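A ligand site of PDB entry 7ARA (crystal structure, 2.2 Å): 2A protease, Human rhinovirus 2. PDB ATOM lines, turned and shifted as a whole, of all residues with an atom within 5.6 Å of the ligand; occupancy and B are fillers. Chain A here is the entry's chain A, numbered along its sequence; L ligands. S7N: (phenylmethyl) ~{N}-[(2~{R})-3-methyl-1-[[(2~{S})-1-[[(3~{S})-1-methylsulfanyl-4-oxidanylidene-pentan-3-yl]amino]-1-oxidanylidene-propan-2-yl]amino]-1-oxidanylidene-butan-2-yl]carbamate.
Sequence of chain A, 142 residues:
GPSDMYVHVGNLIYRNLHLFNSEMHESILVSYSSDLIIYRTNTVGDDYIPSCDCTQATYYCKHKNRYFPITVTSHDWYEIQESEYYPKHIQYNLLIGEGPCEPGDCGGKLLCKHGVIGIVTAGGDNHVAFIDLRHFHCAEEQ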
ATOM      1  N   ASN A  16      12.897  20.178  20.345  1.00  0.00           N
ATOM      2  CA  ASN A  16      12.285  19.071  21.071  1.00  0.00           C
ATOM      3  C   ASN A  16      13.320  18.233  21.784  1.00  0.00           C
ATOM      4  O   ASN A  16      14.273  17.756  21.174  1.00  0.00           O
ATOM      5  CB  ASN A  16      11.464  18.204  20.124  1.00  0.00           C
ATOM      6  CG  ASN A  16      10.299  18.936  19.549  1.00  0.00           C
ATOM      7  OD1 ASN A  16      10.381  19.520  18.457  1.00  0.00           O
ATOM      8  ND2 ASN A  16       9.183  18.941  20.279  1.00  0.00           N
ATOM      9  N   HIS A  18      13.285  15.232  22.991  1.00  0.00           N
ATOM     10  CA  HIS A  18      13.399  13.822  22.620  1.00  0.00           C
ATOM     11  C   HIS A  18      14.079  13.597  21.270  1.00  0.00           C
ATOM     12  O   HIS A  18      14.237  12.459  20.835  1.00  0.00           O
ATOM     13  CB  HIS A  18      12.013  13.153  22.618  1.00  0.00           C
ATOM     14  CG  HIS A  18      11.097  13.646  21.536  1.00  0.00           C
ATOM     15  ND1 HIS A  18      11.311  13.397  20.193  1.00  0.00           N
ATOM     16  CD2 HIS A  18       9.935  14.341  21.602  1.00  0.00           C
ATOM     17  CE1 HIS A  18      10.341  13.929  19.482  1.00  0.00           C
ATOM     18  NE2 HIS A  18       9.488  14.506  20.315  1.00  0.00           N
ATOM     19  N   LEU A  19      14.490  14.686  20.618  1.00  0.00           N
ATOM     20  CA  LEU A  19      15.141  14.575  19.320  1.00  0.00           C
ATOM     21  C   LEU A  19      16.572  15.109  19.348  1.00  0.00           C
ATOM     22  O   LEU A  19      17.392  14.764  18.501  1.00  0.00           O
ATOM     23  CB  LEU A  19      14.348  15.318  18.245  1.00  0.00           C
ATOM     24  CG  LEU A  19      13.109  14.624  17.677  1.00  0.00           C
ATOM     25  CD1 LEU A  19      12.404  15.507  16.664  1.00  0.00           C
ATOM     26  CD2 LEU A  19      13.476  13.283  17.072  1.00  0.00           C
ATOM     27  N   TYR A  78      -1.422  16.325  29.905  1.00  0.00           N
ATOM     28  CA  TYR A  78      -2.071  15.337  29.064  1.00  0.00           C
ATOM     29  C   TYR A  78      -1.049  14.217  28.869  1.00  0.00           C
ATOM     30  O   TYR A  78       0.151  14.463  28.936  1.00  0.00           O
ATOM     31  CB  TYR A  78      -2.507  15.952  27.722  1.00  0.00           C
ATOM     32  CG  TYR A  78      -3.340  15.045  26.840  1.00  0.00           C
ATOM     33  CD1 TYR A  78      -2.764  14.001  26.122  1.00  0.00           C
ATOM     34  CD2 TYR A  78      -4.709  15.256  26.698  1.00  0.00           C
ATOM     35  CE1 TYR A  78      -3.522  13.175  25.322  1.00  0.00           C
ATOM     36  CE2 TYR A  78      -5.478  14.449  25.878  1.00  0.00           C
ATOM     37  CZ  TYR A  78      -4.882  13.398  25.196  1.00  0.00           C
ATOM     38  OH  TYR A  78      -5.629  12.587  24.386  1.00  0.00           O
ATOM     39  N   GLU A  79      -1.519  12.997  28.645  1.00  0.00           N
ATOM     40  CA  GLU A  79      -0.606  11.858  28.521  1.00  0.00           C
ATOM     41  C   GLU A  79      -0.647  11.224  27.140  1.00  0.00           C
ATOM     42  O   GLU A  79      -1.670  10.672  26.728  1.00  0.00           O
ATOM     43  CB  GLU A  79      -0.923  10.809  29.596  1.00  0.00           C
ATOM     44  N   ILE A  80       0.482  11.285  26.426  1.00  0.00           N
ATOM     45  CA  ILE A  80       0.615  10.693  25.098  1.00  0.00           C
ATOM     46  C   ILE A  80       0.823   9.174  25.163  1.00  0.00           C
ATOM     47  O   ILE A  80       1.220   8.644  26.195  1.00  0.00           O
ATOM     48  CB  ILE A  80       1.790  11.311  24.324  1.00  0.00           C
ATOM     49  N   GLN A  81       0.554   8.488  24.057  1.00  0.00           N
ATOM     50  CA  GLN A  81       0.705   7.024  23.993  1.00  0.00           C
ATOM     51  C   GLN A  81       2.131   6.593  23.666  1.00  0.00           C
ATOM     52  O   GLN A  81       3.079   7.373  23.809  1.00  0.00           O
ATOM     53  CB  GLN A  81      -0.251   6.415  22.967  1.00  0.00           C
ATOM     54  CG  GLN A  81      -1.558   5.906  23.544  1.00  0.00           C
ATOM     55  CD  GLN A  81      -2.285   6.946  24.374  1.00  0.00           C
ATOM     56  OE1 GLN A  81      -2.447   8.085  23.948  1.00  0.00           O
ATOM     57  NE2 GLN A  81      -2.719   6.556  25.568  1.00  0.00           N
ATOM     58  N   GLU A  82       2.270   5.355  23.225  1.00  0.00           N
ATOM     59  CA  GLU A  82       3.599   4.780  22.992  1.00  0.00           C
ATOM     60  C   GLU A  82       3.832   4.463  21.521  1.00  0.00           C
ATOM     61  O   GLU A  82       3.064   3.724  20.903  1.00  0.00           O
ATOM     62  CB  GLU A  82       3.778   3.509  23.828  1.00  0.00           C
ATOM     63  N   SER A  83       4.903   5.019  20.972  1.00  0.00           N
ATOM     64  CA  SER A  83       5.315   4.699  19.608  1.00  0.00           C
ATOM     65  C   SER A  83       6.419   3.642  19.630  1.00  0.00           C
ATOM     66  O   SER A  83       6.345   2.684  20.400  1.00  0.00           O
ATOM     67  CB  SER A  83       5.796   5.943  18.868  1.00  0.00           C
ATOM     68  OG  SER A  83       6.793   6.630  19.614  1.00  0.00           O
ATOM     69  N   TYR A  85       9.374   4.396  20.455  1.00  0.00           N
ATOM     70  CA  TYR A  85      10.294   4.856  21.482  1.00  0.00           C
ATOM     71  C   TYR A  85       9.503   5.670  22.507  1.00  0.00           C
ATOM     72  O   TYR A  85       8.425   6.178  22.204  1.00  0.00           O
ATOM     73  CB  TYR A  85      11.424   5.698  20.893  1.00  0.00           C
ATOM     74  CG  TYR A  85      11.079   7.153  20.676  1.00  0.00           C
ATOM     75  CD1 TYR A  85      11.353   8.104  21.648  1.00  0.00           C
ATOM     76  CD2 TYR A  85      10.499   7.572  19.496  1.00  0.00           C
ATOM     77  CE1 TYR A  85      11.036   9.427  21.469  1.00  0.00           C
ATOM     78  CE2 TYR A  85      10.185   8.899  19.288  1.00  0.00           C
ATOM     79  CZ  TYR A  85      10.459   9.818  20.278  1.00  0.00           C
ATOM     80  OH  TYR A  85      10.147  11.133  20.084  1.00  0.00           O
ATOM     81  N   HIS A  89       3.926   8.259  28.036  1.00  0.00           N
ATOM     82  CA  HIS A  89       4.333   9.174  29.091  1.00  0.00           C
ATOM     83  C   HIS A  89       3.336  10.317  29.227  1.00  0.00           C
ATOM     84  O   HIS A  89       2.452  10.485  28.398  1.00  0.00           O
ATOM     85  CB  HIS A  89       5.739   9.724  28.809  1.00  0.00           C
ATOM     86  CG  HIS A  89       5.815  10.640  27.619  1.00  0.00           C
ATOM     87  ND1 HIS A  89       5.284  11.913  27.617  1.00  0.00           N
ATOM     88  CD2 HIS A  89       6.375  10.473  26.397  1.00  0.00           C
ATOM     89  CE1 HIS A  89       5.509  12.486  26.448  1.00  0.00           C
ATOM     90  NE2 HIS A  89       6.168  11.630  25.688  1.00  0.00           N
ATOM     91  N   ILE A  96      -3.099  22.214  22.588  1.00  0.00           N
ATOM     92  CA  ILE A  96      -3.664  21.227  21.685  1.00  0.00           C
ATOM     93  C   ILE A  96      -4.827  21.818  20.894  1.00  0.00           C
ATOM     94  O   ILE A  96      -5.674  22.514  21.441  1.00  0.00           O
ATOM     95  CB  ILE A  96      -4.140  19.961  22.438  1.00  0.00           C
ATOM     96  CG1 ILE A  96      -3.001  19.340  23.252  1.00  0.00           C
ATOM     97  CG2 ILE A  96      -4.676  18.935  21.470  1.00  0.00           C
ATOM     98  CD1 ILE A  96      -3.378  18.047  23.948  1.00  0.00           C
ATOM     99  N   GLU A 102       1.814  13.832  11.497  1.00  0.00           N
ATOM    100  CA  GLU A 102       2.492  12.546  11.343  1.00  0.00           C
ATOM    101  C   GLU A 102       3.955  12.671  11.750  1.00  0.00           C
ATOM    102  O   GLU A 102       4.503  13.768  11.710  1.00  0.00           O
ATOM    103  CB  GLU A 102       2.370  12.059   9.897  1.00  0.00           C
ATOM    104  CG  GLU A 102       1.082  11.339   9.607  1.00  0.00           C
ATOM    105  CD  GLU A 102       1.180  10.475   8.373  1.00  0.00           C
ATOM    106  OE1 GLU A 102       2.317  10.179   7.949  1.00  0.00           O
ATOM    107  OE2 GLU A 102       0.123  10.069   7.838  1.00  0.00           O
ATOM    108  N   PRO A 103       4.577  11.555  12.160  1.00  0.00           N
ATOM    109  CA  PRO A 103       5.989  11.538  12.552  1.00  0.00           C
ATOM    110  C   PRO A 103       6.890  12.363  11.634  1.00  0.00           C
ATOM    111  O   PRO A 103       6.764  12.311  10.410  1.00  0.00           O
ATOM    112  CB  PRO A 103       6.342  10.056  12.481  1.00  0.00           C
ATOM    113  CG  PRO A 103       5.086   9.386  12.910  1.00  0.00           C
ATOM    114  CD  PRO A 103       3.950  10.240  12.381  1.00  0.00           C
ATOM    115  N   GLY A 104       7.790  13.145  12.237  1.00  0.00           N
ATOM    116  CA  GLY A 104       8.699  14.001  11.496  1.00  0.00           C
ATOM    117  C   GLY A 104       8.240  15.448  11.450  1.00  0.00           C
ATOM    118  O   GLY A 104       8.905  16.299  10.851  1.00  0.00           O
ATOM    119  N   ASP A 105       7.106  15.728  12.088  1.00  0.00           N
ATOM    120  CA  ASP A 105       6.486  17.042  11.994  1.00  0.00           C
ATOM    121  C   ASP A 105       6.881  17.989  13.116  1.00  0.00           C
ATOM    122  O   ASP A 105       6.481  19.157  13.110  1.00  0.00           O
ATOM    123  CB  ASP A 105       4.963  16.899  11.972  1.00  0.00           C
ATOM    124  CG  ASP A 105       4.412  16.660  10.576  1.00  0.00           C
ATOM    125  OD1 ASP A 105       5.172  16.833   9.603  1.00  0.00           O
ATOM    126  OD2 ASP A 105       3.218  16.314  10.469  1.00  0.00           O
ATOM    127  N   CYS A 106       7.665  17.505  14.069  1.00  0.00           N
ATOM    128  CA  CYS A 106       8.013  18.318  15.234  1.00  0.00           C
ATOM    129  C   CYS A 106       9.046  19.378  14.982  1.00  0.00           C
ATOM    130  O   CYS A 106       9.905  19.258  14.108  1.00  0.00           O
ATOM    131  CB  CYS A 106       8.471  17.441  16.377  1.00  0.00           C
ATOM    132  SG  CYS A 106       7.097  16.613  17.118  1.00  0.00           S
ATOM    133  N   VAL A 120       5.620  21.900  17.529  1.00  0.00           N
ATOM    134  CA  VAL A 120       4.971  20.603  17.563  1.00  0.00           C
ATOM    135  C   VAL A 120       5.766  19.623  18.425  1.00  0.00           C
ATOM    136  O   VAL A 120       6.993  19.574  18.333  1.00  0.00           O
ATOM    137  CB  VAL A 120       4.803  20.036  16.139  1.00  0.00           C
ATOM    138  CG1 VAL A 120       4.117  18.684  16.183  1.00  0.00           C
ATOM    139  CG2 VAL A 120       4.000  21.011  15.297  1.00  0.00           C
ATOM    140  N   THR A 121       5.074  18.881  19.277  1.00  0.00           N
ATOM    141  CA  THR A 121       5.721  17.897  20.135  1.00  0.00           C
ATOM    142  C   THR A 121       5.049  16.530  20.022  1.00  0.00           C
ATOM    143  O   THR A 121       5.716  15.486  20.087  1.00  0.00           O
ATOM    144  CB  THR A 121       5.714  18.329  21.609  1.00  0.00           C
ATOM    145  OG1 THR A 121       6.094  17.229  22.445  1.00  0.00           O
ATOM    146  CG2 THR A 121       4.335  18.833  22.015  1.00  0.00           C
ATOM    147  N   ALA A 122       3.735  16.521  19.824  1.00  0.00           N
ATOM    148  CA  ALA A 122       2.981  15.283  19.738  1.00  0.00           C
ATOM    149  C   ALA A 122       1.855  15.388  18.709  1.00  0.00           C
ATOM    150  O   ALA A 122       1.293  16.455  18.500  1.00  0.00           O
ATOM    151  CB  ALA A 122       2.417  14.912  21.099  1.00  0.00           C
ATOM    152  N   GLY A 123       1.528  14.266  18.091  1.00  0.00           N
ATOM    153  CA  GLY A 123       0.500  14.244  17.073  1.00  0.00           C
ATOM    154  C   GLY A 123      -0.278  12.942  17.026  1.00  0.00           C
ATOM    155  O   GLY A 123       0.287  11.854  17.111  1.00  0.00           O
ATOM    156  N   GLY A 124      -1.599  13.063  16.900  1.00  0.00           N
ATOM    157  CA  GLY A 124      -2.452  11.905  16.862  1.00  0.00           C
ATOM    158  C   GLY A 124      -3.639  12.076  15.954  1.00  0.00           C
ATOM    159  O   GLY A 124      -3.574  12.756  14.922  1.00  0.00           O
ATOM    160  N   ASP A 125      -4.752  11.444  16.347  1.00  0.00           N
ATOM    161  CA  ASP A 125      -5.972  11.468  15.563  1.00  0.00           C
ATOM    162  C   ASP A 125      -6.540  12.876  15.428  1.00  0.00           C
ATOM    163  O   ASP A 125      -7.261  13.345  16.308  1.00  0.00           O
ATOM    164  CB  ASP A 125      -7.012  10.537  16.187  1.00  0.00           C
ATOM    165  CG  ASP A 125      -6.579   9.096  16.187  1.00  0.00           C
ATOM    166  OD1 ASP A 125      -6.305   8.563  15.084  1.00  0.00           O
ATOM    167  OD2 ASP A 125      -6.502   8.490  17.266  1.00  0.00           O
ATOM    168  N   HIS A 127      -5.452  15.589  15.959  1.00  0.00           N
ATOM    169  CA  HIS A 127      -5.067  16.495  17.032  1.00  0.00           C
ATOM    170  C   HIS A 127      -3.556  16.555  17.115  1.00  0.00           C
ATOM    171  O   HIS A 127      -2.872  15.536  17.064  1.00  0.00           O
ATOM    172  CB  HIS A 127      -5.677  16.048  18.364  1.00  0.00           C
ATOM    173  CG  HIS A 127      -7.123  16.412  18.517  1.00  0.00           C
ATOM    174  ND1 HIS A 127      -8.138  15.550  18.199  1.00  0.00           N
ATOM    175  CD2 HIS A 127      -7.703  17.561  18.946  1.00  0.00           C
ATOM    176  CE1 HIS A 127      -9.303  16.147  18.432  1.00  0.00           C
ATOM    177  NE2 HIS A 127      -9.067  17.358  18.878  1.00  0.00           N
ATOM    178  N   VAL A 128      -3.035  17.778  17.237  1.00  0.00           N
ATOM    179  CA  VAL A 128      -1.602  17.993  17.314  1.00  0.00           C
ATOM    180  C   VAL A 128      -1.255  18.821  18.553  1.00  0.00           C
ATOM    181  O   VAL A 128      -1.864  19.858  18.808  1.00  0.00           O
ATOM    182  CB  VAL A 128      -1.069  18.685  16.037  1.00  0.00           C
ATOM    183  CG1 VAL A 128      -1.950  19.873  15.655  1.00  0.00           C
ATOM    184  CG2 VAL A 128       0.383  19.118  16.227  1.00  0.00           C
ATOM    185  N   ALA A 129      -0.280  18.339  19.328  1.00  0.00           N
ATOM    186  CA  ALA A 129       0.124  19.007  20.562  1.00  0.00           C
ATOM    187  C   ALA A 129       1.371  19.868  20.348  1.00  0.00           C
ATOM    188  O   ALA A 129       2.273  19.501  19.594  1.00  0.00           O
ATOM    189  CB  ALA A 129       0.371  17.991  21.657  1.00  0.00           C
HETATM  190  C10 S7N L   1       7.009  11.020  20.429  1.00  0.00           C
HETATM  191  C20 S7N L   1      -1.732  12.977  20.751  1.00  0.00           C
HETATM  192  C21 S7N L   1      -2.438  13.857  19.903  1.00  0.00           C
HETATM  193  C22 S7N L   1      -2.994  15.028  20.423  1.00  0.00           C
HETATM  194  C24 S7N L   1      -2.144  14.450  22.606  1.00  0.00           C
HETATM  195  C26 S7N L   1       2.510   8.756  18.778  1.00  0.00           C
HETATM  196  C28 S7N L   1       3.079   7.924  19.931  1.00  0.00           C
HETATM  197  C01 S7N L   1      10.925   8.301  14.964  1.00  0.00           C
HETATM  198  C03 S7N L   1       9.784  10.852  15.768  1.00  0.00           C
HETATM  199  C04 S7N L   1       8.682  11.900  15.459  1.00  0.00           C
HETATM  200  C05 S7N L   1       8.594  12.877  16.642  1.00  0.00           C
HETATM  201  C07 S7N L   1       6.751  11.406  17.892  1.00  0.00           C
HETATM  202  C09 S7N L   1       6.039  11.373  19.296  1.00  0.00           C
HETATM  203  C12 S7N L   1       3.614  11.066  19.135  1.00  0.00           C
HETATM  204  C14 S7N L   1       2.322  10.205  19.158  1.00  0.00           C
HETATM  205  C16 S7N L   1       0.384   9.913  20.840  1.00  0.00           C
HETATM  206  C19 S7N L   1      -1.119  11.690  20.195  1.00  0.00           C
HETATM  207  C23 S7N L   1      -2.850  15.331  21.757  1.00  0.00           C
HETATM  208  C25 S7N L   1      -1.595  13.276  22.091  1.00  0.00           C
HETATM  209  C27 S7N L   1       3.262   8.553  17.445  1.00  0.00           C
HETATM  210  C29 S7N L   1       8.013  14.252  16.324  1.00  0.00           C
HETATM  211  C30 S7N L   1       7.660  15.052  17.592  1.00  0.00           C
HETATM  212  N06 S7N L   1       7.759  12.490  17.754  1.00  0.00           N
HETATM  213  N11 S7N L   1       4.896  10.486  19.326  1.00  0.00           N
HETATM  214  N15 S7N L   1       1.802  10.268  20.531  1.00  0.00           N
HETATM  215  O08 S7N L   1       6.481  10.585  17.022  1.00  0.00           O
HETATM  216  O13 S7N L   1       3.526  12.252  18.960  1.00  0.00           O
HETATM  217  O17 S7N L   1       0.002   8.745  20.719  1.00  0.00           O
HETATM  218  O18 S7N L   1      -0.521  10.946  21.276  1.00  0.00           O
HETATM  219  O31 S7N L   1       7.816  14.664  15.201  1.00  0.00           O
HETATM  220  S02 S7N L   1       9.921   9.692  14.440  1.00  0.00           S
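The backbone NH (N) of Cys 106 lies within hydrogen-bond range of an oxygen (O31) of the ligand (3.1 Å).
N of Gly 123 sits at hydrogen-bond distance from O13 of the ligand (3.0 Å).
SG of Cys 106 is covalently linked to C30 of the ligand, 1.7 Å away.
The backbone NH (N) of Asp 105 lies within hydrogen-bond range of an oxygen (O31) of the ligand, at 3.4 Å.
N of Gln 81 sits close to O17 of the ligand (3.4 Å).
The backbone NH of Gly 104 is in hydrogen-bond range of an oxygen (O31) of the ligand.
The backbone NH (N) of Thr 121 lies within hydrogen-bond range of the backbone carbonyl oxygen (O) of Ala 129.
The backbone carbonyl oxygen (O) of Ala 122 sits at hydrogen-bond distance from the backbone NH (N) of Ala 129 (2.6 Å).
OD2 of Asp 105 lies within hydrogen-bond range of N of Glu 102, 3.0 Å away.
ND1 of His 127 lies within hydrogen-bond range of O of Asp 125.
The side-chain sulfur of Cys 106 lies close to the backbone NH of Thr 121, 3.7 Å away.
The backbone NH (N) of Ile 80 is in hydrogen-bond range of the backbone carbonyl oxygen (O) of His 89, 2.9 Å away.
The side-chain hydroxyl (OG) of Ser 83 lies within hydrogen-bond range of the backbone carbonyl oxygen (O) of Tyr 85 (3.1 Å).
ND1 of His 18 sits at hydrogen-bond distance from OH of Tyr 85.
His 18 touches the ligand.
Tyr 78 touches the ligand (CE1 to C24, 3.3 Å).
Ile 80 touches the ligand.
Glu 82 touches the ligand (C to C28, 3.9 Å).
Ser 83 touches the ligand (CB to C28, 3.5 Å).
Tyr 85 touches the ligand (OH to C10, 3.2 Å).
Ile 96 touches the ligand.
Pro 103 touches the ligand.
Thr 121 touches the ligand.
CA of Ala 122 touches O13 of the ligand, 3.2 Å away.
Gly 124 touches the ligand.
His 127 touches the ligand.
Hydrophobic or aromatic side chains that line the ligand: His 18, Tyr 78, Ile 80, Tyr 85, Ile 96, Ala 122 and His 127.
17 residues have an atom within 4 Å of the ligand: His 18, Tyr 78, Ile 80, Gln 81, Glu 82, Ser 83, Tyr 85, Ile 96, Pro 103, Gly 104, Asp 105, Cys 106, Thr 121, Ala 122, Gly 123, Gly 124 and His 127.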
